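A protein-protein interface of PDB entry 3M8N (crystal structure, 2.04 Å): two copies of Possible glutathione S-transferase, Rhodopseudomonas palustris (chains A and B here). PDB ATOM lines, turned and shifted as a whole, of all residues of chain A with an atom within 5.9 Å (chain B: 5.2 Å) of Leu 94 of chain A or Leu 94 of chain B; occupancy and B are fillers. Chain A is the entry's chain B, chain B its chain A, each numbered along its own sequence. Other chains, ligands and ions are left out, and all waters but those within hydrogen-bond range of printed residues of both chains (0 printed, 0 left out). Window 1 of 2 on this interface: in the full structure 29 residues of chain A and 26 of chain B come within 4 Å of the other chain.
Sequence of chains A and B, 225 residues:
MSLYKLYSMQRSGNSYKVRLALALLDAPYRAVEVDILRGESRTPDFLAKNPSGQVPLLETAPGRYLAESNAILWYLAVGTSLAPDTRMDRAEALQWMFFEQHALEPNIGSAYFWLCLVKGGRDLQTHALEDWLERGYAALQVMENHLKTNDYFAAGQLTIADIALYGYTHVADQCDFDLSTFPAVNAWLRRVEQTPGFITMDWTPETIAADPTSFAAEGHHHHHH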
ATOM      1  N   GLU A  68     -15.204  32.281 -30.601  1.00  0.00           N
ATOM      2  CA  GLU A  68     -15.162  31.020 -29.834  1.00  0.00           C
ATOM      3  C   GLU A  68     -16.305  30.093 -30.286  1.00  0.00           C
ATOM      4  O   GLU A  68     -17.481  30.381 -30.107  1.00  0.00           O
ATOM      5  CB  GLU A  68     -15.189  31.268 -28.316  1.00  0.00           C
ATOM      6  CG  GLU A  68     -13.920  31.878 -27.751  1.00  0.00           C
ATOM      7  CD  GLU A  68     -12.745  30.978 -27.810  1.00  0.00           C
ATOM      8  OE1 GLU A  68     -12.910  29.745 -27.938  1.00  0.00           O
ATOM      9  OE2 GLU A  68     -11.611  31.486 -27.711  1.00  0.00           O
ATOM     10  N   ALA A  71     -19.006  29.187 -27.753  1.00  0.00           N
ATOM     11  CA  ALA A  71     -19.816  30.313 -27.408  1.00  0.00           C
ATOM     12  C   ALA A  71     -20.792  30.635 -28.520  1.00  0.00           C
ATOM     13  O   ALA A  71     -21.914  30.984 -28.278  1.00  0.00           O
ATOM     14  CB  ALA A  71     -18.950  31.518 -27.117  1.00  0.00           C
ATOM     15  N   TRP A  74     -23.580  28.101 -28.214  1.00  0.00           N
ATOM     16  CA  TRP A  74     -24.467  28.437 -27.177  1.00  0.00           C
ATOM     17  C   TRP A  74     -25.390  29.523 -27.627  1.00  0.00           C
ATOM     18  O   TRP A  74     -26.583  29.436 -27.429  1.00  0.00           O
ATOM     19  CB  TRP A  74     -23.673  28.860 -25.948  1.00  0.00           C
ATOM     20  CG  TRP A  74     -24.537  29.224 -24.761  1.00  0.00           C
ATOM     21  CD1 TRP A  74     -25.079  30.419 -24.470  1.00  0.00           C
ATOM     22  CD2 TRP A  74     -24.953  28.336 -23.776  1.00  0.00           C
ATOM     23  NE1 TRP A  74     -25.836  30.336 -23.348  1.00  0.00           N
ATOM     24  CE2 TRP A  74     -25.767  29.053 -22.890  1.00  0.00           C
ATOM     25  CE3 TRP A  74     -24.747  26.953 -23.561  1.00  0.00           C
ATOM     26  CZ2 TRP A  74     -26.373  28.450 -21.763  1.00  0.00           C
ATOM     27  CZ3 TRP A  74     -25.378  26.322 -22.419  1.00  0.00           C
ATOM     28  CH2 TRP A  74     -26.158  27.097 -21.535  1.00  0.00           C
ATOM     29  N   ASP A  89     -29.442  20.971 -16.516  1.00  0.00           N
ATOM     30  CA  ASP A  89     -29.148  20.338 -17.790  1.00  0.00           C
ATOM     31  C   ASP A  89     -28.330  21.230 -18.682  1.00  0.00           C
ATOM     32  O   ASP A  89     -27.419  20.759 -19.356  1.00  0.00           O
ATOM     33  CB  ASP A  89     -30.431  20.035 -18.536  1.00  0.00           C
ATOM     34  CG  ASP A  89     -31.206  18.857 -17.976  1.00  0.00           C
ATOM     35  OD1 ASP A  89     -30.737  18.034 -17.194  1.00  0.00           O
ATOM     36  OD2 ASP A  89     -32.341  18.720 -18.390  1.00  0.00           O
ATOM     37  N   ARG A  90     -28.652  22.515 -18.700  1.00  0.00           N
ATOM     38  CA  ARG A  90     -27.803  23.471 -19.406  1.00  0.00           C
ATOM     39  C   ARG A  90     -26.365  23.558 -18.910  1.00  0.00           C
ATOM     40  O   ARG A  90     -25.458  23.521 -19.680  1.00  0.00           O
ATOM     41  CB  ARG A  90     -28.467  24.831 -19.474  1.00  0.00           C
ATOM     42  CG  ARG A  90     -29.380  24.841 -20.639  1.00  0.00           C
ATOM     43  CD  ARG A  90     -30.701  25.480 -20.401  1.00  0.00           C
ATOM     44  NE  ARG A  90     -30.481  26.827 -20.055  1.00  0.00           N
ATOM     45  CZ  ARG A  90     -31.307  27.581 -19.367  1.00  0.00           C
ATOM     46  NH1 ARG A  90     -30.908  28.827 -19.118  1.00  0.00           N
ATOM     47  NH2 ARG A  90     -32.482  27.132 -18.919  1.00  0.00           N
ATOM     48  N   ALA A  91     -26.181  23.633 -17.611  1.00  0.00           N
ATOM     49  CA  ALA A  91     -24.876  23.568 -17.027  1.00  0.00           C
ATOM     50  C   ALA A  91     -24.126  22.288 -17.398  1.00  0.00           C
ATOM     51  O   ALA A  91     -22.941  22.299 -17.571  1.00  0.00           O
ATOM     52  CB  ALA A  91     -24.954  23.723 -15.522  1.00  0.00           C
ATOM     53  N   GLU A  92     -24.847  21.175 -17.479  1.00  0.00           N
ATOM     54  CA  GLU A  92     -24.298  19.865 -17.803  1.00  0.00           C
ATOM     55  C   GLU A  92     -23.784  19.886 -19.234  1.00  0.00           C
ATOM     56  O   GLU A  92     -22.760  19.371 -19.492  1.00  0.00           O
ATOM     57  CB  GLU A  92     -25.339  18.747 -17.556  1.00  0.00           C
ATOM     58  CG  GLU A  92     -24.715  17.458 -17.526  1.00  0.00           C
ATOM     59  CD  GLU A  92     -25.634  16.209 -17.604  1.00  0.00           C
ATOM     60  OE1 GLU A  92     -26.880  16.263 -17.773  1.00  0.00           O
ATOM     61  OE2 GLU A  92     -25.016  15.113 -17.525  1.00  0.00           O
ATOM     62  N   ALA A  93     -24.457  20.564 -20.129  1.00  0.00           N
ATOM     63  CA  ALA A  93     -23.965  20.758 -21.448  1.00  0.00           C
ATOM     64  C   ALA A  93     -22.713  21.630 -21.481  1.00  0.00           C
ATOM     65  O   ALA A  93     -21.727  21.258 -22.103  1.00  0.00           O
ATOM     66  CB  ALA A  93     -25.058  21.364 -22.346  1.00  0.00           C
ATOM     67  N   LEU A  94     -22.719  22.729 -20.745  1.00  0.00           N
ATOM     68  CA  LEU A  94     -21.523  23.520 -20.609  1.00  0.00           C
ATOM     69  C   LEU A  94     -20.387  22.768 -20.051  1.00  0.00           C
ATOM     70  O   LEU A  94     -19.273  22.957 -20.490  1.00  0.00           O
ATOM     71  CB  LEU A  94     -21.754  24.766 -19.772  1.00  0.00           C
ATOM     72  CG  LEU A  94     -22.507  25.867 -20.519  1.00  0.00           C
ATOM     73  CD1 LEU A  94     -22.953  26.921 -19.582  1.00  0.00           C
ATOM     74  CD2 LEU A  94     -21.727  26.508 -21.623  1.00  0.00           C
ATOM     75  N   GLN A  95     -20.648  21.923 -19.088  1.00  0.00           N
ATOM     76  CA  GLN A  95     -19.602  21.077 -18.550  1.00  0.00           C
ATOM     77  C   GLN A  95     -18.860  20.284 -19.648  1.00  0.00           C
ATOM     78  O   GLN A  95     -17.651  20.252 -19.662  1.00  0.00           O
ATOM     79  CB  GLN A  95     -20.143  20.130 -17.489  1.00  0.00           C
ATOM     80  CG  GLN A  95     -19.141  19.075 -17.026  1.00  0.00           C
ATOM     81  CD  GLN A  95     -19.701  17.954 -16.244  1.00  0.00           C
ATOM     82  OE1 GLN A  95     -20.256  18.105 -15.184  1.00  0.00           O
ATOM     83  NE2 GLN A  95     -19.495  16.797 -16.735  1.00  0.00           N
ATOM     84  N   TRP A  96     -19.569  19.635 -20.541  1.00  0.00           N
ATOM     85  CA  TRP A  96     -18.894  18.865 -21.548  1.00  0.00           C
ATOM     86  C   TRP A  96     -18.224  19.751 -22.616  1.00  0.00           C
ATOM     87  O   TRP A  96     -17.257  19.347 -23.250  1.00  0.00           O
ATOM     88  CB  TRP A  96     -19.868  17.876 -22.189  1.00  0.00           C
ATOM     89  CG  TRP A  96     -20.121  16.718 -21.282  1.00  0.00           C
ATOM     90  CD1 TRP A  96     -21.210  16.542 -20.477  1.00  0.00           C
ATOM     91  CD2 TRP A  96     -19.221  15.648 -20.961  1.00  0.00           C
ATOM     92  NE1 TRP A  96     -21.074  15.412 -19.723  1.00  0.00           N
ATOM     93  CE2 TRP A  96     -19.870  14.834 -20.002  1.00  0.00           C
ATOM     94  CE3 TRP A  96     -17.949  15.255 -21.443  1.00  0.00           C
ATOM     95  CZ2 TRP A  96     -19.299  13.661 -19.498  1.00  0.00           C
ATOM     96  CZ3 TRP A  96     -17.389  14.086 -20.949  1.00  0.00           C
ATOM     97  CH2 TRP A  96     -18.084  13.293 -19.989  1.00  0.00           C
ATOM     98  N   MET A  97     -18.792  20.925 -22.874  1.00  0.00           N
ATOM     99  CA  MET A  97     -18.189  21.901 -23.753  1.00  0.00           C
ATOM    100  C   MET A  97     -16.884  22.471 -23.224  1.00  0.00           C
ATOM    101  O   MET A  97     -15.936  22.592 -23.955  1.00  0.00           O
ATOM    102  CB  MET A  97     -19.182  22.996 -24.088  1.00  0.00           C
ATOM    103  CG  MET A  97     -20.270  22.499 -24.884  1.00  0.00           C
ATOM    104  SD  MET A  97     -21.725  23.723 -25.012  1.00  0.00           S
ATOM    105  CE  MET A  97     -21.179  24.433 -26.659  1.00  0.00           C
ATOM    106  N   PHE A  98     -16.821  22.801 -21.954  1.00  0.00           N
ATOM    107  CA  PHE A  98     -15.563  23.193 -21.367  1.00  0.00           C
ATOM    108  C   PHE A  98     -14.488  22.092 -21.356  1.00  0.00           C
ATOM    109  O   PHE A  98     -13.351  22.371 -21.629  1.00  0.00           O
ATOM    110  CB  PHE A  98     -15.800  23.800 -19.977  1.00  0.00           C
ATOM    111  CG  PHE A  98     -16.318  25.219 -20.046  1.00  0.00           C
ATOM    112  CD1 PHE A  98     -15.508  26.249 -20.516  1.00  0.00           C
ATOM    113  CD2 PHE A  98     -17.616  25.521 -19.700  1.00  0.00           C
ATOM    114  CE1 PHE A  98     -16.013  27.525 -20.630  1.00  0.00           C
ATOM    115  CE2 PHE A  98     -18.111  26.807 -19.789  1.00  0.00           C
ATOM    116  CZ  PHE A  98     -17.326  27.807 -20.266  1.00  0.00           C
ATOM    117  N   PHE A  99     -14.870  20.860 -21.023  1.00  0.00           N
ATOM    118  CA  PHE A  99     -14.079  19.649 -21.177  1.00  0.00           C
ATOM    119  C   PHE A  99     -13.521  19.525 -22.589  1.00  0.00           C
ATOM    120  O   PHE A  99     -12.379  19.269 -22.764  1.00  0.00           O
ATOM    121  CB  PHE A  99     -14.957  18.433 -20.884  1.00  0.00           C
ATOM    122  CG  PHE A  99     -14.279  17.116 -21.156  1.00  0.00           C
ATOM    123  CD1 PHE A  99     -13.396  16.557 -20.234  1.00  0.00           C
ATOM    124  CD2 PHE A  99     -14.508  16.428 -22.330  1.00  0.00           C
ATOM    125  CE1 PHE A  99     -12.791  15.348 -20.501  1.00  0.00           C
ATOM    126  CE2 PHE A  99     -13.861  15.212 -22.599  1.00  0.00           C
ATOM    127  CZ  PHE A  99     -13.032  14.696 -21.671  1.00  0.00           C
ATOM    128  N   ALA A 161     -23.718  20.266 -26.612  1.00  0.00           N
ATOM    129  CA  ALA A 161     -22.598  19.552 -26.079  1.00  0.00           C
ATOM    130  C   ALA A 161     -22.174  18.406 -26.981  1.00  0.00           C
ATOM    131  O   ALA A 161     -21.002  18.165 -27.117  1.00  0.00           O
ATOM    132  CB  ALA A 161     -22.869  19.084 -24.740  1.00  0.00           C
ATOM    133  N   ALA B  71     -18.185  25.820 -15.984  1.00  0.00           N
ATOM    134  CA  ALA B  71     -19.590  25.395 -15.955  1.00  0.00           C
ATOM    135  C   ALA B  71     -20.249  25.606 -14.581  1.00  0.00           C
ATOM    136  O   ALA B  71     -21.401  25.962 -14.504  1.00  0.00           O
ATOM    137  CB  ALA B  71     -19.732  23.907 -16.381  1.00  0.00           C
ATOM    138  N   TRP B  74     -21.040  29.346 -14.355  1.00  0.00           N
ATOM    139  CA  TRP B  74     -22.258  29.659 -15.064  1.00  0.00           C
ATOM    140  C   TRP B  74     -23.528  29.262 -14.283  1.00  0.00           C
ATOM    141  O   TRP B  74     -24.471  30.043 -14.205  1.00  0.00           O
ATOM    142  CB  TRP B  74     -22.243  29.016 -16.445  1.00  0.00           C
ATOM    143  CG  TRP B  74     -23.468  29.365 -17.231  1.00  0.00           C
ATOM    144  CD1 TRP B  74     -23.608  30.397 -18.119  1.00  0.00           C
ATOM    145  CD2 TRP B  74     -24.735  28.694 -17.197  1.00  0.00           C
ATOM    146  NE1 TRP B  74     -24.855  30.405 -18.639  1.00  0.00           N
ATOM    147  CE2 TRP B  74     -25.580  29.369 -18.103  1.00  0.00           C
ATOM    148  CE3 TRP B  74     -25.227  27.541 -16.526  1.00  0.00           C
ATOM    149  CZ2 TRP B  74     -26.963  28.956 -18.330  1.00  0.00           C
ATOM    150  CZ3 TRP B  74     -26.584  27.124 -16.741  1.00  0.00           C
ATOM    151  CH2 TRP B  74     -27.437  27.853 -17.636  1.00  0.00           C
ATOM    152  N   ARG B  90     -24.440  37.679 -22.510  1.00  0.00           N
ATOM    153  CA  ARG B  90     -24.203  36.377 -22.020  1.00  0.00           C
ATOM    154  C   ARG B  90     -23.229  35.552 -22.867  1.00  0.00           C
ATOM    155  O   ARG B  90     -22.406  34.860 -22.328  1.00  0.00           O
ATOM    156  CB  ARG B  90     -25.548  35.679 -21.875  1.00  0.00           C
ATOM    157  CG  ARG B  90     -26.374  36.307 -20.850  1.00  0.00           C
ATOM    158  CD  ARG B  90     -27.653  35.582 -20.828  1.00  0.00           C
ATOM    159  NE  ARG B  90     -28.535  36.175 -19.867  1.00  0.00           N
ATOM    160  CZ  ARG B  90     -29.856  36.014 -19.910  1.00  0.00           C
ATOM    161  NH1 ARG B  90     -30.399  35.257 -20.849  1.00  0.00           N
ATOM    162  NH2 ARG B  90     -30.637  36.596 -19.030  1.00  0.00           N
ATOM    163  N   ALA B  91     -23.350  35.605 -24.187  1.00  0.00           N
ATOM    164  CA  ALA B  91     -22.526  34.806 -25.083  1.00  0.00           C
ATOM    165  C   ALA B  91     -21.090  35.329 -25.061  1.00  0.00           C
ATOM    166  O   ALA B  91     -20.161  34.561 -25.113  1.00  0.00           O
ATOM    167  CB  ALA B  91     -23.104  34.830 -26.488  1.00  0.00           C
ATOM    168  N   GLU B  92     -20.904  36.640 -24.910  1.00  0.00           N
ATOM    169  CA  GLU B  92     -19.582  37.215 -24.724  1.00  0.00           C
ATOM    170  C   GLU B  92     -18.925  36.849 -23.456  1.00  0.00           C
ATOM    171  O   GLU B  92     -17.763  36.646 -23.469  1.00  0.00           O
ATOM    172  CB  GLU B  92     -19.588  38.748 -24.805  1.00  0.00           C
ATOM    173  CG  GLU B  92     -20.054  39.294 -26.118  1.00  0.00           C
ATOM    174  CD  GLU B  92     -20.010  40.835 -26.151  1.00  0.00           C
ATOM    175  OE1 GLU B  92     -19.805  41.509 -25.076  1.00  0.00           O
ATOM    176  OE2 GLU B  92     -20.177  41.361 -27.278  1.00  0.00           O
ATOM    177  N   ALA B  93     -19.658  36.751 -22.356  1.00  0.00           N
ATOM    178  CA  ALA B  93     -19.112  36.211 -21.110  1.00  0.00           C
ATOM    179  C   ALA B  93     -18.591  34.820 -21.308  1.00  0.00           C
ATOM    180  O   ALA B  93     -17.542  34.526 -20.821  1.00  0.00           O
ATOM    181  CB  ALA B  93     -20.152  36.235 -19.973  1.00  0.00           C
ATOM    182  N   LEU B  94     -19.346  33.960 -22.013  1.00  0.00           N
ATOM    183  CA  LEU B  94     -18.949  32.595 -22.310  1.00  0.00           C
ATOM    184  C   LEU B  94     -17.799  32.559 -23.251  1.00  0.00           C
ATOM    185  O   LEU B  94     -16.926  31.756 -23.094  1.00  0.00           O
ATOM    186  CB  LEU B  94     -20.137  31.754 -22.872  1.00  0.00           C
ATOM    187  CG  LEU B  94     -21.177  31.298 -21.834  1.00  0.00           C
ATOM    188  CD1 LEU B  94     -22.457  30.890 -22.472  1.00  0.00           C
ATOM    189  CD2 LEU B  94     -20.689  30.258 -20.793  1.00  0.00           C
ATOM    190  N   GLN B  95     -17.808  33.447 -24.246  1.00  0.00           N
ATOM    191  CA  GLN B  95     -16.675  33.625 -25.159  1.00  0.00           C
ATOM    192  C   GLN B  95     -15.387  33.791 -24.380  1.00  0.00           C
ATOM    193  O   GLN B  95     -14.474  33.024 -24.569  1.00  0.00           O
ATOM    194  CB  GLN B  95     -16.885  34.803 -26.056  1.00  0.00           C
ATOM    195  CG  GLN B  95     -15.722  35.062 -26.921  1.00  0.00           C
ATOM    196  CD  GLN B  95     -15.720  36.425 -27.567  1.00  0.00           C
ATOM    197  OE1 GLN B  95     -16.574  36.789 -28.374  1.00  0.00           O
ATOM    198  NE2 GLN B  95     -14.685  37.155 -27.288  1.00  0.00           N
ATOM    199  N   TRP B  96     -15.348  34.734 -23.444  1.00  0.00           N
ATOM    200  CA  TRP B  96     -14.167  34.924 -22.659  1.00  0.00           C
ATOM    201  C   TRP B  96     -13.850  33.760 -21.741  1.00  0.00           C
ATOM    202  O   TRP B  96     -12.712  33.477 -21.487  1.00  0.00           O
ATOM    203  CB  TRP B  96     -14.250  36.238 -21.906  1.00  0.00           C
ATOM    204  CG  TRP B  96     -14.058  37.383 -22.830  1.00  0.00           C
ATOM    205  CD1 TRP B  96     -15.005  38.233 -23.282  1.00  0.00           C
ATOM    206  CD2 TRP B  96     -12.841  37.778 -23.443  1.00  0.00           C
ATOM    207  NE1 TRP B  96     -14.461  39.135 -24.143  1.00  0.00           N
ATOM    208  CE2 TRP B  96     -13.127  38.871 -24.269  1.00  0.00           C
ATOM    209  CE3 TRP B  96     -11.521  37.305 -23.387  1.00  0.00           C
ATOM    210  CZ2 TRP B  96     -12.143  39.505 -25.050  1.00  0.00           C
ATOM    211  CZ3 TRP B  96     -10.539  37.943 -24.177  1.00  0.00           C
ATOM    212  CH2 TRP B  96     -10.860  39.023 -24.975  1.00  0.00           C
ATOM    213  N   MET B  97     -14.843  33.071 -21.192  1.00  0.00           N
ATOM    214  CA  MET B  97     -14.571  31.836 -20.453  1.00  0.00           C
ATOM    215  C   MET B  97     -14.071  30.664 -21.287  1.00  0.00           C
ATOM    216  O   MET B  97     -13.282  29.862 -20.799  1.00  0.00           O
ATOM    217  CB  MET B  97     -15.829  31.386 -19.730  1.00  0.00           C
ATOM    218  CG  MET B  97     -16.384  32.442 -18.910  1.00  0.00           C
ATOM    219  SD  MET B  97     -17.935  31.958 -17.814  1.00  0.00           S
ATOM    220  CE  MET B  97     -16.982  30.992 -16.654  1.00  0.00           C
ATOM    221  N   PHE B  98     -14.569  30.522 -22.511  1.00  0.00           N
ATOM    222  CA  PHE B  98     -13.997  29.555 -23.423  1.00  0.00           C
ATOM    223  C   PHE B  98     -12.575  29.924 -23.789  1.00  0.00           C
ATOM    224  O   PHE B  98     -11.743  29.051 -23.838  1.00  0.00           O
ATOM    225  CB  PHE B  98     -14.876  29.321 -24.645  1.00  0.00           C
ATOM    226  CG  PHE B  98     -16.052  28.420 -24.353  1.00  0.00           C
ATOM    227  CD1 PHE B  98     -15.847  27.121 -23.946  1.00  0.00           C
ATOM    228  CD2 PHE B  98     -17.361  28.899 -24.403  1.00  0.00           C
ATOM    229  CE1 PHE B  98     -16.930  26.253 -23.664  1.00  0.00           C
ATOM    230  CE2 PHE B  98     -18.442  28.070 -24.060  1.00  0.00           C
ATOM    231  CZ  PHE B  98     -18.200  26.723 -23.722  1.00  0.00           C
ATOM    232  N   PHE B  99     -12.300  31.218 -23.953  1.00  0.00           N
ATOM    233  CA  PHE B  99     -10.955  31.716 -24.156  1.00  0.00           C
ATOM    234  C   PHE B  99     -10.102  31.385 -23.006  1.00  0.00           C
ATOM    235  O   PHE B  99      -9.025  30.927 -23.225  1.00  0.00           O
ATOM    236  CB  PHE B  99     -10.969  33.206 -24.392  1.00  0.00           C
ATOM    237  CG  PHE B  99      -9.598  33.874 -24.373  1.00  0.00           C
ATOM    238  CD1 PHE B  99      -8.853  34.007 -25.519  1.00  0.00           C
ATOM    239  CD2 PHE B  99      -9.113  34.465 -23.211  1.00  0.00           C
ATOM    240  CE1 PHE B  99      -7.620  34.673 -25.472  1.00  0.00           C
ATOM    241  CE2 PHE B  99      -7.896  35.118 -23.200  1.00  0.00           C
ATOM    242  CZ  PHE B  99      -7.168  35.211 -24.304  1.00  0.00           C
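Of the 12 printed residues of chain B, 8 touch a printed residue of chain A. Hydrophobic or aromatic side chains of chain B that line the printed part of chain A: Ala 71, Trp 74, Leu 94, Met 97, Phe 98 and Phe 99. Printed residues of chain A that touch a printed residue of chain B: Glu 68, Ala 71, Trp 74, Arg 90, Ala 91, Leu 94, Gln 95, Met 97 and Phe 98. Among the printed residues, no Asp or Glu carboxylate lies within 4 Å of a Lys or Arg side-chain nitrogen of the other chain.
Of the printed residues of chain B, Arg 90 of chain A touches Trp 74 (3.7 Å). Of chain B, only Ala 71 (3.9 Å), Trp 74 (3.4 Å) and Leu 94 (3.98 Å) come within 4 Å of Leu 94 of chain A. Ala 161 of chain A touches none of the printed residues of chain B. Printed residues of chain A within 4 Å of Ala 71 of chain B: Ala 91 (3.8 Å), Leu 94 (3.9 Å), Gln 95 (3.5 Å) and Phe 98 (3.8 Å). Leu 94 of chain B touches just these residues of chain A: Trp 74 and Leu 94. Printed residues of chain A within 4 Å of Phe 99 of chain B: Glu 68 (3.6 Å).
Ala 91 of chain B touches Ala 71 of chain A (O to CB, 3.8 Å). Ala 71 of chain A touches Gln 95 of chain B (CB to N, 3.6 Å). Ala 71 of chain A touches Phe 98 of chain B (N to CD2, 3.7 Å). Arg 90 of chain A touches Trp 74 of chain B (CB to CH2, 3.7 Å). Ala 91 of chain A touches Ala 71 of chain B (O to CB, 3.8 Å). N of Ala 91 of chain A touches CZ3 of Trp 74 of chain B, 3.6 Å away. Leu 94 of chain A touches Ala 71 of chain B. Leu 94 of chain A touches Trp 74 of chain B. Ala 71 of chain B touches Gln 95 of chain A. Phe 98 of chain A touches Met 97 of chain B (CE1 to O, 3.6 Å).
Ala 71 of chain A touches Ala 91 of chain B, and with the chains exchanged Ala 91 of chain A touches Ala 71 of chain B. Ala 91 of chain A touches Trp 74 of chain B, but with the chains exchanged Trp 74 of chain A does not touch Ala 91 of chain B (5.1 Å). Leu 94 of chain A touches Ala 71 of chain B, but with the chains exchanged Ala 71 of chain A does not touch Leu 94 of chain B (4.2 Å). Leu 94 of chain A touches its own counterpart, Leu 94 of chain B. Of the 19 pairs that touch across the chains among the printed residues, 13 have their exchanged pair printed and touching as well.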
